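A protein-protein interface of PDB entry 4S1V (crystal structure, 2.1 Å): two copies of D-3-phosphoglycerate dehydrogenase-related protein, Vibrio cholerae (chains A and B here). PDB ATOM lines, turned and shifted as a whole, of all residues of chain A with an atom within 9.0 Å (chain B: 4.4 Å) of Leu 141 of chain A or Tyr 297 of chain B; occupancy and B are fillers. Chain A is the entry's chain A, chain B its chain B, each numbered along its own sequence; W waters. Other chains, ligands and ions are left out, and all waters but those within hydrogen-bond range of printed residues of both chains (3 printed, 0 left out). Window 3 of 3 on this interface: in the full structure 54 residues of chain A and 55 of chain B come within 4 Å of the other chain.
No position is printed for both chains.
Of the 13 pairs that touch across the chains among the printed residues, none has its exchanged pair printed and touching as well.
The side-chain hydroxyl of Thr 144 of chain A sits at hydrogen-bond distance from the side-chain amide nitrogen of Asn 295 of chain B (2.6 Å).
The side-chain carboxylate of Glu 293 of chain B sits at hydrogen-bond distance from the backbone NH of Thr 144 of chain A (2.9 Å).
N of Lys 294 of chain B sits at hydrogen-bond distance from O of Gly 142 of chain A (2.8 Å).
O of Val 292 of chain B lies within hydrogen-bond range of NH2 of Arg 119 of chain A, at 3.1 Å.
The side-chain amide oxygen of Gln 134 of chain A is in hydrogen-bond range of the guanidinium group of Arg 57 of chain B, 3.0 Å away.
Of chain B, only Val 13 (3.8 Å), Val 292 (3.7 Å), Lys 294 (3.96 Å) and Tyr 297 (3.8 Å) come within 4 Å of Leu 141 of chain A.
Of chain A, only Leu 141 comes within 4 Å of Tyr 297 of chain B.
Val 292 of chain B touches three residues of chain A.
No residue of chain A comes within 4 Å of Ser 296 of chain B.
Of the printed residues of chain A, Glu 293 of chain B touches Arg 119, Gly 142, Arg 143 and Thr 144.
Of the printed residues of chain A, Arg 57 of chain B touches Gln 134 (3.0 Å).
Printed residues of chain B within 4 Å of Gln 134 of chain A: Arg 57 (3.0 Å) and Val 292 (3.5 Å).
Printed residues of chain A within 4 Å of Asn 295 of chain B: Thr 144.
Of the printed residues of chain B, Arg 143 of chain A touches Glu 293.
Tyr 124 of chain A touches none of the printed residues of chain B.
Ile 54 of chain B touches none of the printed residues of chain A.
The nearest printed residue of chain A that does not touch Val 13 of chain B is Gly 140 of chain A (4.7 Å).
Of the 16 printed residues of chain B, 7 touch a printed residue of chain A.
Hydrophobic or aromatic side chains of chain B within 4 Å of the printed part of chain A: Val 13, Val 292 and Tyr 297.
Along chain B the printed residues that touch a printed residue of chain A span positions 13 to 297.
Of the 18 printed residues of chain A, 6 touch a printed residue of chain B.
Water W1 lies within hydrogen-bond range of the backbone carbonyl oxygen of Val 292 of chain B (2.6 Å), the backbone NH of Gly 142 of chain A (2.8 Å) and the side-chain hydroxyl of Tyr 124 of chain A (3.1 Å).
Water W3 lies within hydrogen-bond range of NE of Arg 119 of chain A (2.7 Å) and O of Val 292 of chain B (3.3 Å).
Water W2 lies within hydrogen-bond range of the side-chain hydroxyl of Tyr 291 of chain B (2.8 Å), the guanidinium group of Arg 57 of chain B (2.8 Å) and the side-chain amide nitrogen of Gln 134 of chain A (2.9 Å).
Among the printed residues, merely in contact across the chains: Arg 143 of chain A with Glu 293 of chain B (3.3 Å), Gln 134 of chain A with Val 292 of chain B (3.5 Å), Arg 119 of chain A with Glu 293 of chain B (3.6 Å), Gly 142 of chain A with Glu 293 of chain B (3.7 Å), Leu 141 of chain A with Val 292 of chain B (3.7 Å), Leu 141 of chain A with Val 13 of chain B (3.8 Å), Leu 141 of chain A with Tyr 297 of chain B (3.8 Å) and Leu 141 of chain A with Lys 294 of chain B (3.96 Å).
The guanidinium group (NH1) of Arg 143 of chain A lies within salt-bridge range of the side-chain carboxylate (OD2) of Asp 231 of chain A.
NH2 of Arg 57 of chain B lies within hydrogen-bond range of OH of Tyr 297 of chain B, at 3.0 Å.
OE2 of Glu 298 of chain B is in salt-bridge range of NZ of Lys 294 of chain B.
The side-chain hydroxyl of Tyr 291 of chain B sits at hydrogen-bond distance from the guanidinium group of Arg 57 of chain B (3.0 Å).
The side-chain carboxylate of Glu 293 of chain B lies within hydrogen-bond range of the backbone NH of Ser 296 of chain B (2.7 Å).
OE2 of Glu 293 of chain B lies within hydrogen-bond range of N of Asn 295 of chain B (2.9 Å).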
ATOM      1  N   ALA A 117     -12.758  -5.622 -28.822  1.00  0.00           N
ATOM      2  CA  ALA A 117     -11.676  -5.099 -29.656  1.00  0.00           C
ATOM      3  C   ALA A 117     -11.815  -3.585 -29.821  1.00  0.00           C
ATOM      4  O   ALA A 117     -10.874  -2.854 -29.556  1.00  0.00           O
ATOM      5  CB  ALA A 117     -11.661  -5.793 -31.010  1.00  0.00           C
ATOM      6  N   SER A 118     -12.999  -3.130 -30.233  1.00  0.00           N
ATOM      7  CA  SER A 118     -13.298  -1.698 -30.421  1.00  0.00           C
ATOM      8  C   SER A 118     -12.992  -0.842 -29.190  1.00  0.00           C
ATOM      9  O   SER A 118     -12.639   0.323 -29.326  1.00  0.00           O
ATOM     10  CB  SER A 118     -14.764  -1.489 -30.806  1.00  0.00           C
ATOM     11  OG  SER A 118     -15.113  -2.203 -31.979  1.00  0.00           O
ATOM     12  N   ARG A 119     -13.139  -1.417 -28.001  1.00  0.00           N
ATOM     13  CA  ARG A 119     -12.901  -0.682 -26.750  1.00  0.00           C
ATOM     14  C   ARG A 119     -11.649  -1.114 -25.963  1.00  0.00           C
ATOM     15  O   ARG A 119     -11.399  -0.585 -24.878  1.00  0.00           O
ATOM     16  CB  ARG A 119     -14.145  -0.746 -25.847  1.00  0.00           C
ATOM     17  CG  ARG A 119     -15.412  -0.159 -26.465  1.00  0.00           C
ATOM     18  CD  ARG A 119     -15.249   1.306 -26.876  1.00  0.00           C
ATOM     19  NE  ARG A 119     -15.189   2.177 -25.704  1.00  0.00           N
ATOM     20  CZ  ARG A 119     -16.233   2.802 -25.171  1.00  0.00           C
ATOM     21  NH1 ARG A 119     -17.445   2.681 -25.710  1.00  0.00           N
ATOM     22  NH2 ARG A 119     -16.061   3.563 -24.099  1.00  0.00           N
ATOM     23  N   HIS A 120     -10.881  -2.065 -26.507  1.00  0.00           N
ATOM     24  CA  HIS A 120      -9.667  -2.589 -25.867  1.00  0.00           C
ATOM     25  C   HIS A 120      -9.925  -3.030 -24.454  1.00  0.00           C
ATOM     26  O   HIS A 120      -9.103  -2.810 -23.573  1.00  0.00           O
ATOM     27  CB  HIS A 120      -8.516  -1.573 -25.922  1.00  0.00           C
ATOM     28  CG  HIS A 120      -8.337  -0.937 -27.275  1.00  0.00           C
ATOM     29  ND1 HIS A 120      -8.094  -1.657 -28.384  1.00  0.00           N
ATOM     30  CD2 HIS A 120      -8.412   0.392 -27.677  1.00  0.00           C
ATOM     31  CE1 HIS A 120      -8.001  -0.839 -29.443  1.00  0.00           C
ATOM     32  NE2 HIS A 120      -8.195   0.420 -29.014  1.00  0.00           N
ATOM     33  N   LEU A 121     -11.075  -3.669 -24.251  1.00  0.00           N
ATOM     34  CA  LEU A 121     -11.558  -4.077 -22.931  1.00  0.00           C
ATOM     35  C   LEU A 121     -10.673  -5.071 -22.154  1.00  0.00           C
ATOM     36  O   LEU A 121     -10.360  -4.811 -20.992  1.00  0.00           O
ATOM     37  CB  LEU A 121     -12.992  -4.599 -23.034  1.00  0.00           C
ATOM     38  CG  LEU A 121     -13.718  -4.979 -21.742  1.00  0.00           C
ATOM     39  CD1 LEU A 121     -13.827  -3.801 -20.776  1.00  0.00           C
ATOM     40  CD2 LEU A 121     -15.092  -5.542 -22.079  1.00  0.00           C
ATOM     41  N   TYR A 124      -7.567  -3.255 -20.904  1.00  0.00           N
ATOM     42  CA  TYR A 124      -7.894  -2.343 -19.817  1.00  0.00           C
ATOM     43  C   TYR A 124      -8.099  -3.091 -18.502  1.00  0.00           C
ATOM     44  O   TYR A 124      -7.693  -2.606 -17.443  1.00  0.00           O
ATOM     45  CB  TYR A 124      -9.149  -1.531 -20.135  1.00  0.00           C
ATOM     46  CG  TYR A 124      -8.951  -0.225 -20.885  1.00  0.00           C
ATOM     47  CD1 TYR A 124      -8.245   0.845 -20.314  1.00  0.00           C
ATOM     48  CD2 TYR A 124      -9.538  -0.029 -22.143  1.00  0.00           C
ATOM     49  CE1 TYR A 124      -8.094   2.049 -20.998  1.00  0.00           C
ATOM     50  CE2 TYR A 124      -9.399   1.173 -22.827  1.00  0.00           C
ATOM     51  CZ  TYR A 124      -8.687   2.208 -22.251  1.00  0.00           C
ATOM     52  OH  TYR A 124      -8.561   3.396 -22.944  1.00  0.00           O
ATOM     53  N   TRP A 133      -4.278   2.271 -13.519  1.00  0.00           N
ATOM     54  CA  TRP A 133      -5.636   2.763 -13.749  1.00  0.00           C
ATOM     55  C   TRP A 133      -5.863   3.349 -15.116  1.00  0.00           C
ATOM     56  O   TRP A 133      -5.236   4.346 -15.497  1.00  0.00           O
ATOM     57  CB  TRP A 133      -6.002   3.776 -12.676  1.00  0.00           C
ATOM     58  CG  TRP A 133      -7.369   4.378 -12.881  1.00  0.00           C
ATOM     59  CD1 TRP A 133      -7.674   5.610 -13.452  1.00  0.00           C
ATOM     60  CD2 TRP A 133      -8.667   3.777 -12.539  1.00  0.00           C
ATOM     61  NE1 TRP A 133      -9.027   5.811 -13.480  1.00  0.00           N
ATOM     62  CE2 TRP A 133      -9.686   4.751 -12.940  1.00  0.00           C
ATOM     63  CE3 TRP A 133      -9.070   2.578 -11.958  1.00  0.00           C
ATOM     64  CZ2 TRP A 133     -11.046   4.512 -12.768  1.00  0.00           C
ATOM     65  CZ3 TRP A 133     -10.445   2.349 -11.780  1.00  0.00           C
ATOM     66  CH2 TRP A 133     -11.407   3.296 -12.176  1.00  0.00           C
ATOM     67  N   GLN A 134      -6.772   2.727 -15.868  1.00  0.00           N
ATOM     68  CA  GLN A 134      -7.179   3.199 -17.198  1.00  0.00           C
ATOM     69  C   GLN A 134      -6.011   3.205 -18.196  1.00  0.00           C
ATOM     70  O   GLN A 134      -5.776   4.179 -18.908  1.00  0.00           O
ATOM     71  CB  GLN A 134      -7.851   4.575 -17.117  1.00  0.00           C
ATOM     72  CG  GLN A 134      -8.776   4.882 -18.280  1.00  0.00           C
ATOM     73  CD  GLN A 134      -9.634   6.104 -18.027  1.00  0.00           C
ATOM     74  OE1 GLN A 134      -9.300   7.208 -18.451  1.00  0.00           O
ATOM     75  NE2 GLN A 134     -10.744   5.912 -17.332  1.00  0.00           N
ATOM     76  N   ASN A 136      -4.117   0.377 -21.149  1.00  0.00           N
ATOM     77  CA  ASN A 136      -4.466  -0.793 -21.963  1.00  0.00           C
ATOM     78  C   ASN A 136      -3.281  -1.343 -22.761  1.00  0.00           C
ATOM     79  O   ASN A 136      -3.468  -2.009 -23.773  1.00  0.00           O
ATOM     80  CB  ASN A 136      -5.621  -0.450 -22.906  1.00  0.00           C
ATOM     81  CG  ASN A 136      -5.319   0.730 -23.801  1.00  0.00           C
ATOM     82  OD1 ASN A 136      -4.166   1.138 -23.957  1.00  0.00           O
ATOM     83  ND2 ASN A 136      -6.365   1.293 -24.405  1.00  0.00           N
ATOM     84  N   GLY A 138      -1.032   0.662 -24.200  1.00  0.00           N
ATOM     85  CA  GLY A 138      -0.714   1.622 -25.261  1.00  0.00           C
ATOM     86  C   GLY A 138      -1.549   1.469 -26.523  1.00  0.00           C
ATOM     87  O   GLY A 138      -1.110   1.832 -27.620  1.00  0.00           O
ATOM     88  N   LEU A 139      -2.759   0.932 -26.376  1.00  0.00           N
ATOM     89  CA  LEU A 139      -3.652   0.774 -27.517  1.00  0.00           C
ATOM     90  C   LEU A 139      -4.475   2.038 -27.789  1.00  0.00           C
ATOM     91  O   LEU A 139      -5.123   2.149 -28.827  1.00  0.00           O
ATOM     92  CB  LEU A 139      -4.552  -0.462 -27.349  1.00  0.00           C
ATOM     93  CG  LEU A 139      -3.851  -1.825 -27.313  1.00  0.00           C
ATOM     94  CD1 LEU A 139      -4.838  -2.963 -27.073  1.00  0.00           C
ATOM     95  CD2 LEU A 139      -3.039  -2.076 -28.582  1.00  0.00           C
ATOM     96  N   GLY A 140      -4.448   2.983 -26.855  1.00  0.00           N
ATOM     97  CA  GLY A 140      -5.103   4.281 -27.039  1.00  0.00           C
ATOM     98  C   GLY A 140      -6.587   4.248 -26.727  1.00  0.00           C
ATOM     99  O   GLY A 140      -7.067   3.326 -26.055  1.00  0.00           O
ATOM    100  N   LEU A 141      -7.308   5.266 -27.195  1.00  0.00           N
ATOM    101  CA  LEU A 141      -8.749   5.369 -26.951  1.00  0.00           C
ATOM    102  C   LEU A 141      -9.486   4.348 -27.785  1.00  0.00           C
ATOM    103  O   LEU A 141      -9.098   4.076 -28.923  1.00  0.00           O
ATOM    104  CB  LEU A 141      -9.283   6.768 -27.289  1.00  0.00           C
ATOM    105  CG  LEU A 141      -8.953   7.934 -26.348  1.00  0.00           C
ATOM    106  CD1 LEU A 141      -9.478   9.243 -26.921  1.00  0.00           C
ATOM    107  CD2 LEU A 141      -9.515   7.709 -24.955  1.00  0.00           C
ATOM    108  N   GLY A 142     -10.547   3.782 -27.218  1.00  0.00           N
ATOM    109  CA  GLY A 142     -11.449   2.942 -27.992  1.00  0.00           C
ATOM    110  C   GLY A 142     -12.318   3.773 -28.923  1.00  0.00           C
ATOM    111  O   GLY A 142     -12.210   5.001 -28.961  1.00  0.00           O
ATOM    112  N   ARG A 143     -13.184   3.104 -29.674  1.00  0.00           N
ATOM    113  CA  ARG A 143     -14.116   3.809 -30.536  1.00  0.00           C
ATOM    114  C   ARG A 143     -15.502   3.173 -30.480  1.00  0.00           C
ATOM    115  O   ARG A 143     -15.637   1.983 -30.190  1.00  0.00           O
ATOM    116  CB  ARG A 143     -13.598   3.885 -31.984  1.00  0.00           C
ATOM    117  CG  ARG A 143     -13.619   2.568 -32.740  1.00  0.00           C
ATOM    118  CD  ARG A 143     -13.450   2.782 -34.237  1.00  0.00           C
ATOM    119  NE  ARG A 143     -13.653   1.541 -34.988  1.00  0.00           N
ATOM    120  CZ  ARG A 143     -13.423   1.402 -36.291  1.00  0.00           C
ATOM    121  NH1 ARG A 143     -12.974   2.422 -37.016  1.00  0.00           N
ATOM    122  NH2 ARG A 143     -13.636   0.234 -36.877  1.00  0.00           N
ATOM    123  N   THR A 144     -16.519   3.980 -30.757  1.00  0.00           N
ATOM    124  CA  THR A 144     -17.893   3.492 -30.858  1.00  0.00           C
ATOM    125  C   THR A 144     -18.169   2.891 -32.221  1.00  0.00           C
ATOM    126  O   THR A 144     -17.527   3.241 -33.216  1.00  0.00           O
ATOM    127  CB  THR A 144     -18.903   4.618 -30.640  1.00  0.00           C
ATOM    128  OG1 THR A 144     -18.417   5.804 -31.280  1.00  0.00           O
ATOM    129  CG2 THR A 144     -19.070   4.882 -29.162  1.00  0.00           C
ATOM    130  N   ASP A 231      -7.609   2.534 -39.765  1.00  0.00           N
ATOM    131  CA  ASP A 231      -8.207   2.364 -38.436  1.00  0.00           C
ATOM    132  C   ASP A 231      -9.331   1.312 -38.426  1.00  0.00           C
ATOM    133  O   ASP A 231     -10.173   1.307 -37.535  1.00  0.00           O
ATOM    134  CB  ASP A 231      -8.692   3.713 -37.875  1.00  0.00           C
ATOM    135  CG  ASP A 231      -9.854   4.303 -38.667  1.00  0.00           C
ATOM    136  OD1 ASP A 231     -10.110   3.858 -39.808  1.00  0.00           O
ATOM    137  OD2 ASP A 231     -10.517   5.221 -38.136  1.00  0.00           O
ATOM    138  N   GLN A 259      -6.456  -2.930 -36.588  1.00  0.00           N
ATOM    139  CA  GLN A 259      -6.751  -3.952 -35.582  1.00  0.00           C
ATOM    140  C   GLN A 259      -7.552  -5.138 -36.124  1.00  0.00           C
ATOM    141  O   GLN A 259      -8.230  -5.035 -37.150  1.00  0.00           O
ATOM    142  CB  GLN A 259      -7.381  -3.346 -34.310  1.00  0.00           C
ATOM    143  CG  GLN A 259      -8.721  -2.632 -34.479  1.00  0.00           C
ATOM    144  CD  GLN A 259      -9.381  -2.265 -33.143  1.00  0.00           C
ATOM    145  OE1 GLN A 259     -10.284  -1.412 -33.093  1.00  0.00           O
ATOM    146  NE2 GLN A 259      -8.941  -2.913 -32.057  1.00  0.00           N
ATOM    147  N   VAL B  13      -4.054  11.388 -24.127  1.00  0.00           N
ATOM    148  CA  VAL B  13      -4.650  11.306 -25.457  1.00  0.00           C
ATOM    149  C   VAL B  13      -5.322  12.614 -25.874  1.00  0.00           C
ATOM    150  O   VAL B  13      -5.577  12.837 -27.057  1.00  0.00           O
ATOM    151  CB  VAL B  13      -5.684  10.156 -25.544  1.00  0.00           C
ATOM    152  CG1 VAL B  13      -4.982   8.806 -25.609  1.00  0.00           C
ATOM    153  CG2 VAL B  13      -6.671  10.216 -24.377  1.00  0.00           C
ATOM    154  N   VAL B  14      -5.615  13.471 -24.897  1.00  0.00           N
ATOM    155  CA  VAL B  14      -6.289  14.747 -25.161  1.00  0.00           C
ATOM    156  C   VAL B  14      -5.499  15.613 -26.155  1.00  0.00           C
ATOM    157  O   VAL B  14      -6.092  16.198 -27.064  1.00  0.00           O
ATOM    158  CB  VAL B  14      -6.644  15.492 -23.849  1.00  0.00           C
ATOM    159  CG1 VAL B  14      -7.072  16.933 -24.117  1.00  0.00           C
ATOM    160  CG2 VAL B  14      -7.741  14.743 -23.104  1.00  0.00           C
ATOM    161  N   LEU B  17      -6.401  14.946 -29.868  1.00  0.00           N
ATOM    162  CA  LEU B  17      -7.766  15.109 -30.385  1.00  0.00           C
ATOM    163  C   LEU B  17      -7.846  16.263 -31.384  1.00  0.00           C
ATOM    164  O   LEU B  17      -7.059  17.208 -31.300  1.00  0.00           O
ATOM    165  CB  LEU B  17      -8.749  15.361 -29.241  1.00  0.00           C
ATOM    166  CG  LEU B  17      -8.830  14.355 -28.089  1.00  0.00           C
ATOM    167  CD1 LEU B  17      -9.759  14.878 -27.011  1.00  0.00           C
ATOM    168  CD2 LEU B  17      -9.282  12.984 -28.576  1.00  0.00           C
ATOM    169  N   ILE B  54     -12.001  16.661 -16.412  1.00  0.00           N
ATOM    170  CA  ILE B  54     -12.537  15.478 -17.068  1.00  0.00           C
ATOM    171  C   ILE B  54     -13.536  14.802 -16.135  1.00  0.00           C
ATOM    172  O   ILE B  54     -13.158  14.103 -15.196  1.00  0.00           O
ATOM    173  CB  ILE B  54     -11.435  14.498 -17.519  1.00  0.00           C
ATOM    174  CG1 ILE B  54     -10.372  15.239 -18.350  1.00  0.00           C
ATOM    175  CG2 ILE B  54     -12.051  13.323 -18.284  1.00  0.00           C
ATOM    176  CD1 ILE B  54      -9.294  14.349 -18.937  1.00  0.00           C
ATOM    177  N   ARG B  57     -13.157  13.108 -12.128  1.00  0.00           N
ATOM    178  CA  ARG B  57     -11.864  12.528 -11.707  1.00  0.00           C
ATOM    179  C   ARG B  57     -11.147  13.300 -10.586  1.00  0.00           C
ATOM    180  O   ARG B  57     -10.331  12.730  -9.863  1.00  0.00           O
ATOM    181  CB  ARG B  57     -10.944  12.352 -12.911  1.00  0.00           C
ATOM    182  CG  ARG B  57     -11.476  11.339 -13.906  1.00  0.00           C
ATOM    183  CD  ARG B  57     -10.644  11.308 -15.171  1.00  0.00           C
ATOM    184  NE  ARG B  57     -11.279  10.468 -16.184  1.00  0.00           N
ATOM    185  CZ  ARG B  57     -10.713  10.101 -17.329  1.00  0.00           C
ATOM    186  NH1 ARG B  57      -9.478  10.485 -17.630  1.00  0.00           N
ATOM    187  NH2 ARG B  57     -11.392   9.335 -18.175  1.00  0.00           N
ATOM    188  N   TYR B 291     -17.398   6.554 -20.684  1.00  0.00           N
ATOM    189  CA  TYR B 291     -17.252   7.762 -21.493  1.00  0.00           C
ATOM    190  C   TYR B 291     -15.886   7.903 -22.179  1.00  0.00           C
ATOM    191  O   TYR B 291     -15.660   8.842 -22.941  1.00  0.00           O
ATOM    192  CB  TYR B 291     -17.589   9.014 -20.661  1.00  0.00           C
ATOM    193  CG  TYR B 291     -16.698   9.271 -19.465  1.00  0.00           C
ATOM    194  CD1 TYR B 291     -15.483   9.950 -19.609  1.00  0.00           C
ATOM    195  CD2 TYR B 291     -17.077   8.871 -18.189  1.00  0.00           C
ATOM    196  CE1 TYR B 291     -14.657  10.192 -18.528  1.00  0.00           C
ATOM    197  CE2 TYR B 291     -16.262   9.125 -17.091  1.00  0.00           C
ATOM    198  CZ  TYR B 291     -15.054   9.787 -17.274  1.00  0.00           C
ATOM    199  OH  TYR B 291     -14.232  10.053 -16.206  1.00  0.00           O
ATOM    200  N   VAL B 292     -14.989   6.960 -21.916  1.00  0.00           N
ATOM    201  CA  VAL B 292     -13.609   7.035 -22.396  1.00  0.00           C
ATOM    202  C   VAL B 292     -13.540   6.403 -23.786  1.00  0.00           C
ATOM    203  O   VAL B 292     -13.404   5.191 -23.922  1.00  0.00           O
ATOM    204  CB  VAL B 292     -12.642   6.347 -21.407  1.00  0.00           C
ATOM    205  CG1 VAL B 292     -11.188   6.518 -21.845  1.00  0.00           C
ATOM    206  CG2 VAL B 292     -12.841   6.918 -20.006  1.00  0.00           C
ATOM    207  N   GLU B 293     -13.634   7.247 -24.810  1.00  0.00           N
ATOM    208  CA  GLU B 293     -13.824   6.799 -26.185  1.00  0.00           C
ATOM    209  C   GLU B 293     -13.507   7.962 -27.133  1.00  0.00           C
ATOM    210  O   GLU B 293     -13.678   9.127 -26.759  1.00  0.00           O
ATOM    211  CB  GLU B 293     -15.267   6.302 -26.349  1.00  0.00           C
ATOM    212  CG  GLU B 293     -15.614   5.675 -27.693  1.00  0.00           C
ATOM    213  CD  GLU B 293     -16.122   6.705 -28.687  1.00  0.00           C
ATOM    214  OE1 GLU B 293     -16.932   7.580 -28.303  1.00  0.00           O
ATOM    215  OE2 GLU B 293     -15.706   6.642 -29.855  1.00  0.00           O
ATOM    216  N   LYS B 294     -13.016   7.648 -28.336  1.00  0.00           N
ATOM    217  CA  LYS B 294     -12.586   8.675 -29.310  1.00  0.00           C
ATOM    218  C   LYS B 294     -13.635   9.768 -29.557  1.00  0.00           C
ATOM    219  O   LYS B 294     -13.414  10.935 -29.199  1.00  0.00           O
ATOM    220  CB  LYS B 294     -12.141   8.029 -30.637  1.00  0.00           C
ATOM    221  CG  LYS B 294     -11.484   8.987 -31.637  1.00  0.00           C
ATOM    222  CD  LYS B 294     -10.073   9.373 -31.207  1.00  0.00           C
ATOM    223  CE  LYS B 294      -9.284  10.059 -32.314  1.00  0.00           C
ATOM    224  NZ  LYS B 294      -9.712  11.468 -32.555  1.00  0.00           N
ATOM    225  N   ASN B 295     -14.769   9.382 -30.151  1.00  0.00           N
ATOM    226  CA  ASN B 295     -15.872  10.305 -30.448  1.00  0.00           C
ATOM    227  C   ASN B 295     -16.395  11.045 -29.220  1.00  0.00           C
ATOM    228  O   ASN B 295     -16.579  12.259 -29.253  1.00  0.00           O
ATOM    229  CB  ASN B 295     -17.033   9.572 -31.141  1.00  0.00           C
ATOM    230  CG  ASN B 295     -16.600   8.852 -32.403  1.00  0.00           C
ATOM    231  OD1 ASN B 295     -15.968   9.436 -33.285  1.00  0.00           O
ATOM    232  ND2 ASN B 295     -16.936   7.568 -32.493  1.00  0.00           N
ATOM    233  N   SER B 296     -16.634  10.301 -28.143  1.00  0.00           N
ATOM    234  CA  SER B 296     -17.019  10.880 -26.850  1.00  0.00           C
ATOM    235  C   SER B 296     -16.051  11.983 -26.357  1.00  0.00           C
ATOM    236  O   SER B 296     -16.486  13.077 -25.984  1.00  0.00           O
ATOM    237  CB  SER B 296     -17.157   9.770 -25.807  1.00  0.00           C
ATOM    238  OG  SER B 296     -17.603  10.289 -24.570  1.00  0.00           O
ATOM    239  N   TYR B 297     -14.752  11.689 -26.371  1.00  0.00           N
ATOM    240  CA  TYR B 297     -13.716  12.678 -26.028  1.00  0.00           C
ATOM    241  C   TYR B 297     -13.689  13.887 -26.969  1.00  0.00           C
ATOM    242  O   TYR B 297     -13.442  15.011 -26.520  1.00  0.00           O
ATOM    243  CB  TYR B 297     -12.327  12.035 -25.981  1.00  0.00           C
ATOM    244  CG  TYR B 297     -11.846  11.605 -24.597  1.00  0.00           C
ATOM    245  CD1 TYR B 297     -12.722  11.028 -23.665  1.00  0.00           C
ATOM    246  CD2 TYR B 297     -10.497  11.745 -24.235  1.00  0.00           C
ATOM    247  CE1 TYR B 297     -12.273  10.630 -22.405  1.00  0.00           C
ATOM    248  CE2 TYR B 297     -10.038  11.340 -22.988  1.00  0.00           C
ATOM    249  CZ  TYR B 297     -10.926  10.781 -22.074  1.00  0.00           C
ATOM    250  OH  TYR B 297     -10.475  10.381 -20.827  1.00  0.00           O
ATOM    251  N   GLU B 298     -13.932  13.673 -28.264  1.00  0.00           N
ATOM    252  CA  GLU B 298     -13.969  14.811 -29.187  1.00  0.00           C
ATOM    253  C   GLU B 298     -15.114  15.758 -28.811  1.00  0.00           C
ATOM    254  O   GLU B 298     -14.929  16.982 -28.794  1.00  0.00           O
ATOM    255  CB  GLU B 298     -14.058  14.387 -30.660  1.00  0.00           C
ATOM    256  CG  GLU B 298     -12.802  13.753 -31.249  1.00  0.00           C
ATOM    257  CD  GLU B 298     -11.640  14.714 -31.486  1.00  0.00           C
ATOM    258  OE1 GLU B 298     -11.720  15.912 -31.141  1.00  0.00           O
ATOM    259  OE2 GLU B 298     -10.616  14.253 -32.032  1.00  0.00           O
ATOM    260  N   ILE B 299     -16.274  15.182 -28.480  1.00  0.00           N
ATOM    261  CA  ILE B 299     -17.448  15.950 -28.058  1.00  0.00           C
ATOM    262  C   ILE B 299     -17.162  16.706 -26.756  1.00  0.00           C
ATOM    263  O   ILE B 299     -17.373  17.921 -26.676  1.00  0.00           O
ATOM    264  CB  ILE B 299     -18.691  15.034 -27.922  1.00  0.00           C
ATOM    265  CG1 ILE B 299     -19.175  14.580 -29.310  1.00  0.00           C
ATOM    266  CG2 ILE B 299     -19.811  15.720 -27.150  1.00  0.00           C
ATOM    267  CD1 ILE B 299     -19.845  13.221 -29.314  1.00  0.00           C
ATOM    268  N   TYR B 300     -16.673  15.987 -25.746  1.00  0.00           N
ATOM    269  CA  TYR B 300     -16.367  16.586 -24.445  1.00  0.00           C
ATOM    270  C   TYR B 300     -15.455  17.794 -24.553  1.00  0.00           C
ATOM    271  O   TYR B 300     -15.731  18.854 -23.991  1.00  0.00           O
ATOM    272  CB  TYR B 300     -15.704  15.573 -23.510  1.00  0.00           C
ATOM    273  CG  TYR B 300     -16.657  14.629 -22.838  1.00  0.00           C
ATOM    274  CD1 TYR B 300     -17.868  15.078 -22.303  1.00  0.00           C
ATOM    275  CD2 TYR B 300     -16.338  13.290 -22.706  1.00  0.00           C
ATOM    276  CE1 TYR B 300     -18.740  14.201 -21.677  1.00  0.00           C
ATOM    277  CE2 TYR B 300     -17.201  12.407 -22.076  1.00  0.00           C
ATOM    278  CZ  TYR B 300     -18.395  12.863 -21.568  1.00  0.00           C
ATOM    279  OH  TYR B 300     -19.227  11.967 -20.946  1.00  0.00           O
ATOM    280  N   PHE B 301     -14.361  17.614 -25.275  1.00  0.00           N
ATOM    281  CA  PHE B 301     -13.336  18.624 -25.312  1.00  0.00           C
ATOM    282  C   PHE B 301     -13.635  19.741 -26.313  1.00  0.00           C
ATOM    283  O   PHE B 301     -13.263  20.881 -26.066  1.00  0.00           O
ATOM    284  CB  PHE B 301     -11.955  17.975 -25.460  1.00  0.00           C
ATOM    285  CG  PHE B 301     -11.562  17.161 -24.251  1.00  0.00           C
ATOM    286  CD1 PHE B 301     -11.029  17.780 -23.118  1.00  0.00           C
ATOM    287  CD2 PHE B 301     -11.777  15.788 -24.216  1.00  0.00           C
ATOM    288  CE1 PHE B 301     -10.685  17.042 -21.994  1.00  0.00           C
ATOM    289  CE2 PHE B 301     -11.436  15.040 -23.092  1.00  0.00           C
ATOM    290  CZ  PHE B 301     -10.893  15.671 -21.978  1.00  0.00           C
HETATM  291  O   HOH W   1     -11.099   4.205 -24.467  1.00  0.00           O
HETATM  292  O   HOH W   2     -12.962   7.610 -16.546  1.00  0.00           O
HETATM  293  O   HOH W   3     -12.947   1.902 -24.191  1.00  0.00           O
